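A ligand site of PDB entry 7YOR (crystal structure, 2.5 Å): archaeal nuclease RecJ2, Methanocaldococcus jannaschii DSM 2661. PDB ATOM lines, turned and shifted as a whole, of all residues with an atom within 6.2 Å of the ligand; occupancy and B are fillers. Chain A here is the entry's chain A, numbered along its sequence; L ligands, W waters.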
ATOM      1  N   HIS A  33      33.890   6.888   6.694  1.00  0.00           N
ATOM      2  CA  HIS A  33      32.819   7.827   6.887  1.00  0.00           C
ATOM      3  C   HIS A  33      31.962   7.373   8.071  1.00  0.00           C
ATOM      4  O   HIS A  33      32.045   6.218   8.529  1.00  0.00           O
ATOM      5  CB  HIS A  33      32.002   7.950   5.603  1.00  0.00           C
ATOM      6  CG  HIS A  33      31.225   9.225   5.502  1.00  0.00           C
ATOM      7  ND1 HIS A  33      29.910   9.274   5.079  1.00  0.00           N
ATOM      8  CD2 HIS A  33      31.574  10.505   5.808  1.00  0.00           C
ATOM      9  CE1 HIS A  33      29.487  10.529   5.127  1.00  0.00           C
ATOM     10  NE2 HIS A  33      30.469  11.284   5.563  1.00  0.00           N
ATOM     11  N   HIS A  34      31.110   8.282   8.561  1.00  0.00           N
ATOM     12  CA  HIS A  34      30.305   8.070   9.759  1.00  0.00           C
ATOM     13  C   HIS A  34      28.892   7.589   9.459  1.00  0.00           C
ATOM     14  O   HIS A  34      28.117   7.387  10.395  1.00  0.00           O
ATOM     15  CB  HIS A  34      30.240   9.353  10.593  1.00  0.00           C
ATOM     16  CG  HIS A  34      29.473  10.467   9.927  1.00  0.00           C
ATOM     17  ND1 HIS A  34      29.752  10.927   8.659  1.00  0.00           N
ATOM     18  CD2 HIS A  34      28.430  11.220  10.373  1.00  0.00           C
ATOM     19  CE1 HIS A  34      28.920  11.895   8.347  1.00  0.00           C
ATOM     20  NE2 HIS A  34      28.105  12.096   9.369  1.00  0.00           N
ATOM     21  N   ASP A  35      28.527   7.395   8.203  1.00  0.00           N
ATOM     22  CA  ASP A  35      27.200   6.860   7.944  1.00  0.00           C
ATOM     23  C   ASP A  35      27.192   5.335   8.118  1.00  0.00           C
ATOM     24  O   ASP A  35      28.228   4.698   8.298  1.00  0.00           O
ATOM     25  CB  ASP A  35      26.726   7.250   6.551  1.00  0.00           C
ATOM     26  CG  ASP A  35      27.543   6.577   5.478  1.00  0.00           C
ATOM     27  OD1 ASP A  35      28.782   6.742   5.497  1.00  0.00           O
ATOM     28  OD2 ASP A  35      26.968   5.836   4.650  1.00  0.00           O
ATOM     29  N   GLU A  62      33.888  12.945   8.983  1.00  0.00           N
ATOM     30  CA  GLU A  62      32.617  13.329   8.364  1.00  0.00           C
ATOM     31  C   GLU A  62      32.798  13.843   6.931  1.00  0.00           C
ATOM     32  O   GLU A  62      32.013  13.498   6.041  1.00  0.00           O
ATOM     33  CB  GLU A  62      31.923  14.374   9.238  1.00  0.00           C
ATOM     34  CG  GLU A  62      32.204  14.199  10.757  1.00  0.00           C
ATOM     35  CD  GLU A  62      31.037  14.572  11.690  1.00  0.00           C
ATOM     36  OE1 GLU A  62      29.876  14.645  11.224  1.00  0.00           O
ATOM     37  OE2 GLU A  62      31.282  14.804  12.895  1.00  0.00           O
ATOM     38  N   HIS A  63      33.832  14.644   6.662  1.00  0.00           N
ATOM     39  CA  HIS A  63      34.188  15.031   5.299  1.00  0.00           C
ATOM     40  C   HIS A  63      35.672  14.796   5.094  1.00  0.00           C
ATOM     41  O   HIS A  63      36.491  15.090   5.977  1.00  0.00           O
ATOM     42  CB  HIS A  63      33.876  16.525   4.971  1.00  0.00           C
ATOM     43  CG  HIS A  63      32.518  17.005   5.413  1.00  0.00           C
ATOM     44  ND1 HIS A  63      31.400  16.968   4.590  1.00  0.00           N
ATOM     45  CD2 HIS A  63      32.106  17.565   6.580  1.00  0.00           C
ATOM     46  CE1 HIS A  63      30.365  17.478   5.231  1.00  0.00           C
ATOM     47  NE2 HIS A  63      30.762  17.836   6.439  1.00  0.00           N
ATOM     48  N   ALA A  87      34.879   4.314   1.493  1.00  0.00           N
ATOM     49  CA  ALA A  87      33.753   5.191   1.192  1.00  0.00           C
ATOM     50  C   ALA A  87      34.184   6.622   0.898  1.00  0.00           C
ATOM     51  O   ALA A  87      33.394   7.562   1.036  1.00  0.00           O
ATOM     52  CB  ALA A  87      32.732   5.176   2.337  1.00  0.00           C
ATOM     53  N   GLN A  92      38.750  12.733  -4.089  1.00  0.00           N
ATOM     54  CA  GLN A  92      39.884  13.432  -3.535  1.00  0.00           C
ATOM     55  C   GLN A  92      41.207  12.856  -4.043  1.00  0.00           C
ATOM     56  O   GLN A  92      42.272  13.155  -3.481  1.00  0.00           O
ATOM     57  CB  GLN A  92      39.817  13.392  -1.997  1.00  0.00           C
ATOM     58  CG  GLN A  92      38.444  13.837  -1.410  1.00  0.00           C
ATOM     59  CD  GLN A  92      37.321  12.761  -1.474  1.00  0.00           C
ATOM     60  OE1 GLN A  92      37.482  11.681  -2.065  1.00  0.00           O
ATOM     61  NE2 GLN A  92      36.178  13.080  -0.876  1.00  0.00           N
ATOM     62  N   HIS A 108      32.895   3.700  -3.712  1.00  0.00           N
ATOM     63  CA  HIS A 108      31.875   3.502  -4.739  1.00  0.00           C
ATOM     64  C   HIS A 108      31.272   4.821  -5.222  1.00  0.00           C
ATOM     65  O   HIS A 108      30.233   4.806  -5.898  1.00  0.00           O
ATOM     66  CB  HIS A 108      30.777   2.565  -4.238  1.00  0.00           C
ATOM     67  CG  HIS A 108      29.958   3.138  -3.132  1.00  0.00           C
ATOM     68  ND1 HIS A 108      30.487   3.957  -2.152  1.00  0.00           N
ATOM     69  CD2 HIS A 108      28.644   3.000  -2.828  1.00  0.00           C
ATOM     70  CE1 HIS A 108      29.541   4.301  -1.309  1.00  0.00           C
ATOM     71  NE2 HIS A 108      28.412   3.735  -1.692  1.00  0.00           N
ATOM     72  N   HIS A 109      31.887   5.968  -4.887  1.00  0.00           N
ATOM     73  CA  HIS A 109      31.528   7.261  -5.438  1.00  0.00           C
ATOM     74  C   HIS A 109      32.138   7.417  -6.831  1.00  0.00           C
ATOM     75  O   HIS A 109      33.203   6.858  -7.105  1.00  0.00           O
ATOM     76  CB  HIS A 109      32.028   8.392  -4.548  1.00  0.00           C
ATOM     77  CG  HIS A 109      31.281   8.505  -3.258  1.00  0.00           C
ATOM     78  ND1 HIS A 109      31.872   8.295  -2.037  1.00  0.00           N
ATOM     79  CD2 HIS A 109      29.977   8.783  -3.013  1.00  0.00           C
ATOM     80  CE1 HIS A 109      30.968   8.445  -1.082  1.00  0.00           C
ATOM     81  NE2 HIS A 109      29.810   8.736  -1.641  1.00  0.00           N
ATOM     82  N   ASP A 167      22.573   2.101   2.700  1.00  0.00           N
ATOM     83  CA  ASP A 167      22.662   2.916   1.490  1.00  0.00           C
ATOM     84  C   ASP A 167      21.477   2.732   0.561  1.00  0.00           C
ATOM     85  O   ASP A 167      21.585   3.058  -0.631  1.00  0.00           O
ATOM     86  CB  ASP A 167      23.961   2.627   0.740  1.00  0.00           C
ATOM     87  CG  ASP A 167      24.992   3.719   0.928  1.00  0.00           C
ATOM     88  OD1 ASP A 167      25.003   4.336   2.033  1.00  0.00           O
ATOM     89  OD2 ASP A 167      25.748   4.008  -0.023  1.00  0.00           O
ATOM     90  N   ARG A 290      25.268   9.493  13.671  1.00  0.00           N
ATOM     91  CA  ARG A 290      24.776  10.864  13.677  1.00  0.00           C
ATOM     92  C   ARG A 290      24.965  11.546  15.031  1.00  0.00           C
ATOM     93  O   ARG A 290      24.897  12.778  15.102  1.00  0.00           O
ATOM     94  CB  ARG A 290      23.298  10.894  13.278  1.00  0.00           C
ATOM     95  CG  ARG A 290      23.019  10.271  11.907  1.00  0.00           C
ATOM     96  CD  ARG A 290      23.769  11.019  10.806  1.00  0.00           C
ATOM     97  NE  ARG A 290      23.661  10.338   9.514  1.00  0.00           N
ATOM     98  CZ  ARG A 290      24.292  10.702   8.405  1.00  0.00           C
ATOM     99  NH1 ARG A 290      25.077  11.766   8.371  1.00  0.00           N
ATOM    100  NH2 ARG A 290      24.114   9.982   7.289  1.00  0.00           N
ATOM    101  N   ILE A 347      19.537  16.392   8.774  1.00  0.00           N
ATOM    102  CA  ILE A 347      19.183  16.997   7.494  1.00  0.00           C
ATOM    103  C   ILE A 347      19.255  15.994   6.349  1.00  0.00           C
ATOM    104  O   ILE A 347      18.475  16.076   5.396  1.00  0.00           O
ATOM    105  CB  ILE A 347      20.061  18.225   7.233  1.00  0.00           C
ATOM    106  CG1 ILE A 347      21.519  17.798   7.062  1.00  0.00           C
ATOM    107  CG2 ILE A 347      19.861  19.262   8.347  1.00  0.00           C
ATOM    108  CD1 ILE A 347      22.363  18.834   6.370  1.00  0.00           C
ATOM    109  N   GLY A 348      20.147  15.015   6.438  1.00  0.00           N
ATOM    110  CA  GLY A 348      20.218  13.994   5.413  1.00  0.00           C
ATOM    111  C   GLY A 348      18.991  13.102   5.413  1.00  0.00           C
ATOM    112  O   GLY A 348      18.319  12.929   4.385  1.00  0.00           O
ATOM    113  N   PHE A 372      25.303  21.263   3.405  1.00  0.00           N
ATOM    114  CA  PHE A 372      24.086  20.882   2.699  1.00  0.00           C
ATOM    115  C   PHE A 372      24.057  19.387   2.415  1.00  0.00           C
ATOM    116  O   PHE A 372      25.101  18.740   2.338  1.00  0.00           O
ATOM    117  CB  PHE A 372      23.956  21.660   1.386  1.00  0.00           C
ATOM    118  CG  PHE A 372      23.803  23.134   1.578  1.00  0.00           C
ATOM    119  CD1 PHE A 372      24.883  23.916   1.973  1.00  0.00           C
ATOM    120  CD2 PHE A 372      22.574  23.757   1.366  1.00  0.00           C
ATOM    121  CE1 PHE A 372      24.740  25.267   2.164  1.00  0.00           C
ATOM    122  CE2 PHE A 372      22.438  25.119   1.551  1.00  0.00           C
ATOM    123  CZ  PHE A 372      23.532  25.878   1.954  1.00  0.00           C
ATOM    124  N   SER A 373      22.835  18.860   2.270  1.00  0.00           N
ATOM    125  CA  SER A 373      22.574  17.452   1.966  1.00  0.00           C
ATOM    126  C   SER A 373      21.410  17.354   0.977  1.00  0.00           C
ATOM    127  O   SER A 373      20.269  17.639   1.334  1.00  0.00           O
ATOM    128  CB  SER A 373      22.248  16.632   3.243  1.00  0.00           C
ATOM    129  OG  SER A 373      23.394  16.299   4.018  1.00  0.00           O
ATOM    130  N   ALA A 374      21.691  16.924  -0.233  1.00  0.00           N
ATOM    131  CA  ALA A 374      20.694  16.866  -1.292  1.00  0.00           C
ATOM    132  C   ALA A 374      20.279  15.424  -1.554  1.00  0.00           C
ATOM    133  O   ALA A 374      21.136  14.532  -1.647  1.00  0.00           O
ATOM    134  CB  ALA A 374      21.248  17.511  -2.570  1.00  0.00           C
ATOM    135  N   ARG A 375      18.981  15.188  -1.697  1.00  0.00           N
ATOM    136  CA  ARG A 375      18.490  13.835  -1.971  1.00  0.00           C
ATOM    137  C   ARG A 375      17.485  13.841  -3.124  1.00  0.00           C
ATOM    138  O   ARG A 375      16.687  14.779  -3.270  1.00  0.00           O
ATOM    139  CB  ARG A 375      17.829  13.199  -0.709  1.00  0.00           C
ATOM    140  CG  ARG A 375      18.730  13.093   0.533  1.00  0.00           C
ATOM    141  CD  ARG A 375      19.929  12.143   0.361  1.00  0.00           C
ATOM    142  NE  ARG A 375      20.729  12.047   1.580  1.00  0.00           N
ATOM    143  CZ  ARG A 375      21.854  12.725   1.801  1.00  0.00           C
ATOM    144  NH1 ARG A 375      22.362  13.548   0.903  1.00  0.00           N
ATOM    145  NH2 ARG A 375      22.487  12.579   2.964  1.00  0.00           N
ATOM    146  N   ASN A 400      33.093  23.402  -1.701  1.00  0.00           N
ATOM    147  CA  ASN A 400      33.379  22.058  -2.158  1.00  0.00           C
ATOM    148  C   ASN A 400      32.117  21.212  -2.043  1.00  0.00           C
ATOM    149  O   ASN A 400      31.383  21.323  -1.047  1.00  0.00           O
ATOM    150  CB  ASN A 400      34.511  21.434  -1.329  1.00  0.00           C
ATOM    151  CG  ASN A 400      34.601  19.937  -1.502  1.00  0.00           C
ATOM    152  OD1 ASN A 400      34.799  19.435  -2.610  1.00  0.00           O
ATOM    153  ND2 ASN A 400      34.468  19.212  -0.399  1.00  0.00           N
ATOM    154  N   GLY A 401      31.855  20.364  -3.041  1.00  0.00           N
ATOM    155  CA  GLY A 401      30.688  19.513  -3.005  1.00  0.00           C
ATOM    156  C   GLY A 401      30.793  18.322  -3.934  1.00  0.00           C
ATOM    157  O   GLY A 401      31.473  18.366  -4.964  1.00  0.00           O
ATOM    158  N   GLY A 402      30.088  17.255  -3.562  1.00  0.00           N
ATOM    159  CA  GLY A 402      30.057  16.042  -4.374  1.00  0.00           C
ATOM    160  C   GLY A 402      29.273  14.935  -3.695  1.00  0.00           C
ATOM    161  O   GLY A 402      28.695  15.109  -2.609  1.00  0.00           O
ATOM    162  N   GLY A 403      29.266  13.785  -4.347  1.00  0.00           N
ATOM    163  CA  GLY A 403      28.606  12.588  -3.834  1.00  0.00           C
ATOM    164  C   GLY A 403      28.151  11.683  -4.983  1.00  0.00           C
ATOM    165  O   GLY A 403      28.876  11.519  -5.971  1.00  0.00           O
ATOM    166  N   HIS A 404      26.964  11.099  -4.815  1.00  0.00           N
ATOM    167  CA  HIS A 404      26.326  10.311  -5.863  1.00  0.00           C
ATOM    168  C   HIS A 404      25.338  11.155  -6.651  1.00  0.00           C
ATOM    169  O   HIS A 404      24.928  12.248  -6.236  1.00  0.00           O
ATOM    170  CB  HIS A 404      25.562   9.107  -5.296  1.00  0.00           C
ATOM    171  CG  HIS A 404      26.348   8.202  -4.391  1.00  0.00           C
ATOM    172  ND1 HIS A 404      27.243   7.266  -4.861  1.00  0.00           N
ATOM    173  CD2 HIS A 404      26.318   8.063  -3.047  1.00  0.00           C
ATOM    174  CE1 HIS A 404      27.752   6.602  -3.834  1.00  0.00           C
ATOM    175  NE2 HIS A 404      27.207   7.066  -2.715  1.00  0.00           N
ATOM    176  N   ALA A 407      22.410  11.280  -4.192  1.00  0.00           N
ATOM    177  CA  ALA A 407      22.608  11.842  -2.853  1.00  0.00           C
ATOM    178  C   ALA A 407      23.994  12.456  -2.759  1.00  0.00           C
ATOM    179  O   ALA A 407      24.986  11.753  -2.979  1.00  0.00           O
ATOM    180  CB  ALA A 407      22.412  10.757  -1.784  1.00  0.00           C
ATOM    181  N   SER A 408      24.061  13.739  -2.412  1.00  0.00           N
ATOM    182  CA  SER A 408      25.320  14.465  -2.373  1.00  0.00           C
ATOM    183  C   SER A 408      25.276  15.539  -1.271  1.00  0.00           C
ATOM    184  O   SER A 408      24.208  15.883  -0.750  1.00  0.00           O
ATOM    185  CB  SER A 408      25.638  15.104  -3.709  1.00  0.00           C
ATOM    186  OG  SER A 408      25.983  14.125  -4.662  1.00  0.00           O
ATOM    187  N   GLY A 409      26.458  16.064  -0.943  1.00  0.00           N
ATOM    188  CA  GLY A 409      26.570  17.102   0.063  1.00  0.00           C
ATOM    189  C   GLY A 409      27.484  18.209  -0.425  1.00  0.00           C
ATOM    190  O   GLY A 409      28.080  18.121  -1.490  1.00  0.00           O
ATOM    191  N   ALA A 410      27.580  19.264   0.390  1.00  0.00           N
ATOM    192  CA  ALA A 410      28.410  20.413   0.040  1.00  0.00           C
ATOM    193  C   ALA A 410      28.570  21.305   1.257  1.00  0.00           C
ATOM    194  O   ALA A 410      27.849  21.171   2.244  1.00  0.00           O
ATOM    195  CB  ALA A 410      27.805  21.209  -1.132  1.00  0.00           C
HETATM  196  C1  LIG L   1      29.363  11.232   0.087  1.00  0.00           C
HETATM  197  C2  LIG L   1      31.721  15.824  -0.773  1.00  0.00           C
HETATM  198  C3  LIG L   1      30.728  15.958   0.262  1.00  0.00           C
HETATM  199  C4  LIG L   1      29.918  14.872   0.518  1.00  0.00           C
HETATM  200  C5  LIG L   1      31.056  13.577  -1.237  1.00  0.00           C
HETATM  201  C6  LIG L   1      29.182  12.598   0.094  1.00  0.00           C
HETATM  202  C7  LIG L   1      27.202  11.765   0.590  1.00  0.00           C
HETATM  203  C8  LIG L   1      28.071  10.686   0.415  1.00  0.00           C
HETATM  204  C9  LIG L   1      25.736  11.877   0.954  1.00  0.00           C
HETATM  205  N1  LIG L   1      30.042  13.684  -0.171  1.00  0.00           N
HETATM  206  N2  LIG L   1      31.881  14.705  -1.498  1.00  0.00           N
HETATM  207  N3  LIG L   1      32.570  16.879  -1.082  1.00  0.00           N
HETATM  208  O1  LIG L   1      31.160  12.539  -1.859  1.00  0.00           O
HETATM  209  O2  LIG L   1      27.868  12.919   0.379  1.00  0.00           O
HETATM  210  O3  LIG L   1      27.750   9.394   0.535  1.00  0.00           O
HETATM  211  O4  LIG L   1      25.577  13.161   1.297  1.00  0.00           O
HETATM  212  O5  LIG L   1      27.563  13.902   3.007  1.00  0.00           O
HETATM  213  O6  LIG L   1      25.372  15.232   2.904  1.00  0.00           O
HETATM  214  O7  LIG L   1      25.373  12.907   3.953  1.00  0.00           O
HETATM  215  P1  LIG L   1      26.055  13.896   3.016  1.00  0.00           P
HETATM  216  O   HOH W   1      26.397  17.857   4.670  1.00  0.00           O
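A nitrogen (N1) of the ligand lies close to the backbone carbonyl oxygen (O) of Gly 402, 3.1 Å away.
O of Phe 372 touches O6 of the ligand, 3.6 Å away.
C of Gly 401 touches N3 of the ligand, at 3.7 Å.
Ser 408 touches the ligand.
Gly 409 touches the ligand (CA to O6, 3.6 Å).
Hydrophobic or aromatic side chains that line the ligand: His 109.
Within 4 Å of the ligand: His 109, Phe 372, Ser 373, Arg 375, Asn 400, Gly 401, Gly 402, Gly 403, Ser 408 and Gly 409.
The nearest printed residue that does not touch the ligand is Ala 407 (4.01 Å).
NE2 of His 404 lies close to NE2 of His 109 (3.3 Å).
NH1 of Arg 375 is in hydrogen-bond range of O of Ser 408.
The backbone NH (N) of Gly 409 lies within hydrogen-bond range of the backbone carbonyl oxygen (O) of Gly 402 (2.9 Å).
The side-chain hydroxyl of Ser 408 lies close to the backbone NH of Gly 403, 3.3 Å away.
O of His 404 sits at hydrogen-bond distance from OG of Ser 408, 2.7 Å away.
The backbone carbonyl oxygen (O) of Ser 408 is in hydrogen-bond range of the backbone NH (N) of Ala 374 (2.8 Å).
The backbone NH (N) of Phe 372 is in hydrogen-bond range of the backbone carbonyl oxygen (O) of Ala 410, at 2.8 Å.
Water W1 lies within hydrogen-bond range of O of Phe 372 (2.8 Å), O6 of the ligand (3.3 Å) and OG of Ser 373 (3.4 Å).
An oxygen (O6) of the ligand sits at hydrogen-bond distance from the side-chain hydroxyl of Ser 373, 2.5 Å away.
NE2 of His 109 is in hydrogen-bond range of O3 of the ligand, at 3.1 Å.
O7 of the ligand lies within salt-bridge range of NH2 of Arg 375 (3.1 Å).
The side-chain amide nitrogen of Asn 400 lies close to a nitrogen (N3) of the ligand (3.1 Å).
N of Gly 403 sits close to O1 of the ligand (3.4 Å).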
